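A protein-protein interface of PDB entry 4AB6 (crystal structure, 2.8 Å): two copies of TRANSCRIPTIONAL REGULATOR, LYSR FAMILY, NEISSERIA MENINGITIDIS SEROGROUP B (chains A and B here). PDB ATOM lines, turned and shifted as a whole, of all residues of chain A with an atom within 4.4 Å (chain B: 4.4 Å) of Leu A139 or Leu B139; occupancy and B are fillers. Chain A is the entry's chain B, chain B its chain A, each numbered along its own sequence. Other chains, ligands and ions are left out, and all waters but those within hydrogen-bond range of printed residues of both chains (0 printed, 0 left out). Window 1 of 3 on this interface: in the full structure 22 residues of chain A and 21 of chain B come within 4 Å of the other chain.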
ATOM      1  N   HIS A  17     -10.004   1.006  16.978  1.00  0.00           N
ATOM      2  CA  HIS A  17     -10.184   2.405  17.385  1.00  0.00           C
ATOM      3  C   HIS A  17     -10.823   3.223  16.261  1.00  0.00           C
ATOM      4  O   HIS A  17     -11.557   4.170  16.552  1.00  0.00           O
ATOM      5  CB  HIS A  17      -8.842   3.033  17.795  1.00  0.00           C
ATOM      6  CG  HIS A  17      -8.183   2.396  18.983  1.00  0.00           C
ATOM      7  ND1 HIS A  17      -7.942   3.113  20.149  1.00  0.00           N
ATOM      8  CD2 HIS A  17      -7.712   1.137  19.142  1.00  0.00           C
ATOM      9  CE1 HIS A  17      -7.344   2.271  20.972  1.00  0.00           C
ATOM     10  NE2 HIS A  17      -7.181   1.074  20.415  1.00  0.00           N
ATOM     11  N   PHE A  20     -14.955   3.836  15.876  1.00  0.00           N
ATOM     12  CA  PHE A  20     -15.549   4.923  16.653  1.00  0.00           C
ATOM     13  C   PHE A  20     -15.943   6.126  15.805  1.00  0.00           C
ATOM     14  O   PHE A  20     -16.991   6.714  16.069  1.00  0.00           O
ATOM     15  CB  PHE A  20     -14.610   5.340  17.792  1.00  0.00           C
ATOM     16  CG  PHE A  20     -14.642   4.428  19.004  1.00  0.00           C
ATOM     17  CD1 PHE A  20     -13.794   3.330  19.091  1.00  0.00           C
ATOM     18  CD2 PHE A  20     -15.503   4.683  20.067  1.00  0.00           C
ATOM     19  CE1 PHE A  20     -13.825   2.490  20.216  1.00  0.00           C
ATOM     20  CE2 PHE A  20     -15.535   3.843  21.188  1.00  0.00           C
ATOM     21  CZ  PHE A  20     -14.698   2.757  21.257  1.00  0.00           C
ATOM     22  N   SER A 137       0.062   4.530  19.882  1.00  0.00           N
ATOM     23  CA  SER A 137      -0.715   5.759  20.002  1.00  0.00           C
ATOM     24  C   SER A 137      -2.200   5.452  19.870  1.00  0.00           C
ATOM     25  O   SER A 137      -2.600   4.723  18.956  1.00  0.00           O
ATOM     26  CB  SER A 137      -0.296   6.776  18.948  1.00  0.00           C
ATOM     27  OG  SER A 137      -0.955   8.007  19.190  1.00  0.00           O
ATOM     28  N   GLU A 138      -3.012   6.013  20.775  1.00  0.00           N
ATOM     29  CA  GLU A 138      -4.465   5.833  20.803  1.00  0.00           C
ATOM     30  C   GLU A 138      -5.171   6.682  19.745  1.00  0.00           C
ATOM     31  O   GLU A 138      -6.280   6.340  19.317  1.00  0.00           O
ATOM     32  CB  GLU A 138      -5.014   6.196  22.189  1.00  0.00           C
ATOM     33  CG  GLU A 138      -4.430   5.364  23.328  1.00  0.00           C
ATOM     34  CD  GLU A 138      -5.222   4.159  23.815  1.00  0.00           C
ATOM     35  OE1 GLU A 138      -6.311   3.876  23.263  1.00  0.00           O
ATOM     36  OE2 GLU A 138      -4.772   3.528  24.798  1.00  0.00           O
ATOM     37  N   LEU A 139      -4.545   7.801  19.347  1.00  0.00           N
ATOM     38  CA  LEU A 139      -5.127   8.757  18.408  1.00  0.00           C
ATOM     39  C   LEU A 139      -4.550   8.672  17.004  1.00  0.00           C
ATOM     40  O   LEU A 139      -3.333   8.636  16.841  1.00  0.00           O
ATOM     41  CB  LEU A 139      -5.007  10.210  18.944  1.00  0.00           C
ATOM     42  CG  LEU A 139      -5.284  10.461  20.433  1.00  0.00           C
ATOM     43  CD1 LEU A 139      -4.792  11.819  20.850  1.00  0.00           C
ATOM     44  CD2 LEU A 139      -6.759  10.300  20.772  1.00  0.00           C
ATOM     45  N   THR A 140      -5.437   8.671  15.991  1.00  0.00           N
ATOM     46  CA  THR A 140      -5.092   8.663  14.568  1.00  0.00           C
ATOM     47  C   THR A 140      -4.369   9.987  14.253  1.00  0.00           C
ATOM     48  O   THR A 140      -3.346   9.991  13.566  1.00  0.00           O
ATOM     49  CB  THR A 140      -6.362   8.489  13.730  1.00  0.00           C
ATOM     50  OG1 THR A 140      -7.010   7.266  14.103  1.00  0.00           O
ATOM     51  CG2 THR A 140      -6.081   8.490  12.249  1.00  0.00           C
ATOM     52  N   ILE A 141      -4.902  11.097  14.810  1.00  0.00           N
ATOM     53  CA  ILE A 141      -4.381  12.462  14.741  1.00  0.00           C
ATOM     54  C   ILE A 141      -2.897  12.460  15.105  1.00  0.00           C
ATOM     55  O   ILE A 141      -2.086  13.063  14.402  1.00  0.00           O
ATOM     56  CB  ILE A 141      -5.306  13.320  15.658  1.00  0.00           C
ATOM     57  CG1 ILE A 141      -6.569  13.737  14.924  1.00  0.00           C
ATOM     58  CG2 ILE A 141      -4.698  14.378  16.568  1.00  0.00           C
ATOM     59  CD1 ILE A 141      -6.431  14.970  13.951  1.00  0.00           C
ATOM     60  N   ALA A 142      -2.550  11.699  16.154  1.00  0.00           N
ATOM     61  CA  ALA A 142      -1.196  11.518  16.654  1.00  0.00           C
ATOM     62  C   ALA A 142      -0.333  10.592  15.797  1.00  0.00           C
ATOM     63  O   ALA A 142       0.870  10.838  15.679  1.00  0.00           O
ATOM     64  CB  ALA A 142      -1.227  11.058  18.100  1.00  0.00           C
ATOM     65  N   ILE A 143      -0.939   9.534  15.195  1.00  0.00           N
ATOM     66  CA  ILE A 143      -0.238   8.589  14.314  1.00  0.00           C
ATOM     67  C   ILE A 143       0.228   9.328  13.054  1.00  0.00           C
ATOM     68  O   ILE A 143       1.388   9.196  12.675  1.00  0.00           O
ATOM     69  CB  ILE A 143      -1.086   7.320  14.009  1.00  0.00           C
ATOM     70  CG1 ILE A 143      -1.168   6.395  15.256  1.00  0.00           C
ATOM     71  CG2 ILE A 143      -0.543   6.551  12.784  1.00  0.00           C
ATOM     72  CD1 ILE A 143      -2.272   5.340  15.249  1.00  0.00           C
ATOM     73  N   PHE B  20      -4.194  17.700  21.796  1.00  0.00           N
ATOM     74  CA  PHE B  20      -3.868  17.077  20.508  1.00  0.00           C
ATOM     75  C   PHE B  20      -4.648  17.663  19.329  1.00  0.00           C
ATOM     76  O   PHE B  20      -4.073  17.817  18.253  1.00  0.00           O
ATOM     77  CB  PHE B  20      -4.061  15.560  20.577  1.00  0.00           C
ATOM     78  CG  PHE B  20      -2.936  14.810  21.244  1.00  0.00           C
ATOM     79  CD1 PHE B  20      -2.938  14.597  22.619  1.00  0.00           C
ATOM     80  CD2 PHE B  20      -1.887  14.287  20.496  1.00  0.00           C
ATOM     81  CE1 PHE B  20      -1.896  13.900  23.238  1.00  0.00           C
ATOM     82  CE2 PHE B  20      -0.852  13.584  21.120  1.00  0.00           C
ATOM     83  CZ  PHE B  20      -0.865  13.395  22.488  1.00  0.00           C
ATOM     84  N   SER B 137     -12.120   6.615  29.140  1.00  0.00           N
ATOM     85  CA  SER B 137     -12.118   6.579  27.681  1.00  0.00           C
ATOM     86  C   SER B 137     -11.057   7.519  27.139  1.00  0.00           C
ATOM     87  O   SER B 137     -10.963   8.662  27.580  1.00  0.00           O
ATOM     88  CB  SER B 137     -13.483   6.946  27.110  1.00  0.00           C
ATOM     89  OG  SER B 137     -13.487   6.742  25.706  1.00  0.00           O
ATOM     90  N   GLU B 138     -10.266   7.039  26.178  1.00  0.00           N
ATOM     91  CA  GLU B 138      -9.193   7.795  25.532  1.00  0.00           C
ATOM     92  C   GLU B 138      -9.731   8.778  24.495  1.00  0.00           C
ATOM     93  O   GLU B 138      -9.078   9.784  24.209  1.00  0.00           O
ATOM     94  CB  GLU B 138      -8.200   6.831  24.853  1.00  0.00           C
ATOM     95  CG  GLU B 138      -7.546   5.835  25.803  1.00  0.00           C
ATOM     96  CD  GLU B 138      -6.172   6.178  26.353  1.00  0.00           C
ATOM     97  OE1 GLU B 138      -5.630   7.260  26.028  1.00  0.00           O
ATOM     98  OE2 GLU B 138      -5.616   5.323  27.080  1.00  0.00           O
ATOM     99  N   LEU B 139     -10.906   8.485  23.918  1.00  0.00           N
ATOM    100  CA  LEU B 139     -11.496   9.304  22.857  1.00  0.00           C
ATOM    101  C   LEU B 139     -12.639  10.184  23.324  1.00  0.00           C
ATOM    102  O   LEU B 139     -13.531   9.711  24.022  1.00  0.00           O
ATOM    103  CB  LEU B 139     -11.958   8.417  21.670  1.00  0.00           C
ATOM    104  CG  LEU B 139     -11.060   7.239  21.234  1.00  0.00           C
ATOM    105  CD1 LEU B 139     -11.800   6.329  20.294  1.00  0.00           C
ATOM    106  CD2 LEU B 139      -9.794   7.715  20.557  1.00  0.00           C
ATOM    107  N   THR B 140     -12.623  11.467  22.907  1.00  0.00           N
ATOM    108  CA  THR B 140     -13.668  12.467  23.195  1.00  0.00           C
ATOM    109  C   THR B 140     -14.947  12.012  22.499  1.00  0.00           C
ATOM    110  O   THR B 140     -16.030  12.058  23.089  1.00  0.00           O
ATOM    111  CB  THR B 140     -13.219  13.854  22.709  1.00  0.00           C
ATOM    112  OG1 THR B 140     -12.000  14.204  23.351  1.00  0.00           O
ATOM    113  CG2 THR B 140     -14.251  14.927  22.955  1.00  0.00           C
ATOM    114  N   ILE B 141     -14.787  11.531  21.245  1.00  0.00           N
ATOM    115  CA  ILE B 141     -15.808  10.970  20.365  1.00  0.00           C
ATOM    116  C   ILE B 141     -16.613   9.920  21.151  1.00  0.00           C
ATOM    117  O   ILE B 141     -17.841   9.931  21.113  1.00  0.00           O
ATOM    118  CB  ILE B 141     -15.211  10.335  19.071  1.00  0.00           C
ATOM    119  CG1 ILE B 141     -13.662  10.400  18.858  1.00  0.00           C
ATOM    120  CG2 ILE B 141     -16.024  10.681  17.842  1.00  0.00           C
ATOM    121  CD1 ILE B 141     -13.035  11.771  18.351  1.00  0.00           C
ATOM    122  N   ALA B 142     -15.895   9.070  21.917  1.00  0.00           N
ATOM    123  CA  ALA B 142     -16.431   8.017  22.763  1.00  0.00           C
ATOM    124  C   ALA B 142     -17.056   8.529  24.060  1.00  0.00           C
ATOM    125  O   ALA B 142     -18.046   7.951  24.506  1.00  0.00           O
ATOM    126  CB  ALA B 142     -15.371   6.973  23.049  1.00  0.00           C
ATOM    127  N   ILE B 143     -16.500   9.608  24.658  1.00  0.00           N
ATOM    128  CA  ILE B 143     -17.033  10.224  25.879  1.00  0.00           C
ATOM    129  C   ILE B 143     -18.408  10.822  25.584  1.00  0.00           C
ATOM    130  O   ILE B 143     -19.341  10.572  26.340  1.00  0.00           O
ATOM    131  CB  ILE B 143     -16.039  11.242  26.514  1.00  0.00           C
ATOM    132  CG1 ILE B 143     -14.841  10.501  27.172  1.00  0.00           C
ATOM    133  CG2 ILE B 143     -16.748  12.177  27.525  1.00  0.00           C
ATOM    134  CD1 ILE B 143     -13.629  11.345  27.469  1.00  0.00           C
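OG of Ser B137 sits at hydrogen-bond distance from O of Leu B139, 3.4 Å away. The backbone carbonyl oxygen of Leu A139 is in hydrogen-bond range of the side-chain hydroxyl of Ser A137.
Phe A20 touches Leu B139, and with the chains exchanged Leu A139 touches Phe B20. Phe A20 touches Ala B142, and with the chains exchanged Ala A142 touches Phe B20. Glu A138 touches Leu B139, but with the chains exchanged Leu A139 does not touch Glu B138 (4.2 Å). Ile A141 touches Phe B20, but with the chains exchanged Phe A20 does not touch Ile B141 (4.5 Å). Of the 8 pairs that touch across the chains among the printed residues, 6 have their exchanged pair printed and touching as well.
Phe A20 touches Leu B139 (CG to CD1, 3.7 Å). CE2 of Phe A20 touches CB of Ala B142, at 3.6 Å. O of Glu A138 touches CD2 of Leu B139, 3.97 Å away. CD1 of Leu A139 touches CG of Phe B20 (3.5 Å). CD2 of Leu B139 touches CD2 of Leu A139, 3.99 Å away. Ile A141 touches Phe B20 (CG2 to O, 3.9 Å). CB of Ala A142 touches CE2 of Phe B20, 3.95 Å away.
Hydrophobic or aromatic side chains of chain B that line the printed part of chain A: Phe B20, Leu B139 and Ala B142. Among the printed residues, 8 pairs touch across the chains.
Of the printed residues of chain B, Phe A20 touches Leu B139 (3.7 Å) and Ala B142 (3.6 Å). Printed residues of chain B within 4 Å of Glu A138: Glu B138 (3.0 Å) and Leu B139 (3.97 Å). Of the printed residues of chain B, Leu A139 touches Phe B20 and Leu B139. Of the printed residues of chain B, Ile A141 touches Phe B20. Of the printed residues of chain A, Phe B20 touches Leu A139 (3.5 Å), Ile A141 (3.9 Å) and Ala A142 (3.95 Å). Of the printed residues of chain A, Leu B139 touches Phe A20, Glu A138 and Leu A139. Printed residues of chain A within 4 Å of Ala B142: Phe A20. The nearest printed residue of chain A that does not touch Leu B139 is His A17 (4.3 Å). The nearest printed residue of chain B that does not touch Ala A142 is Leu B139 (9.4 Å).
OE2 of Glu B138 lies close to OE2 of Glu A138 (3.0 Å).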
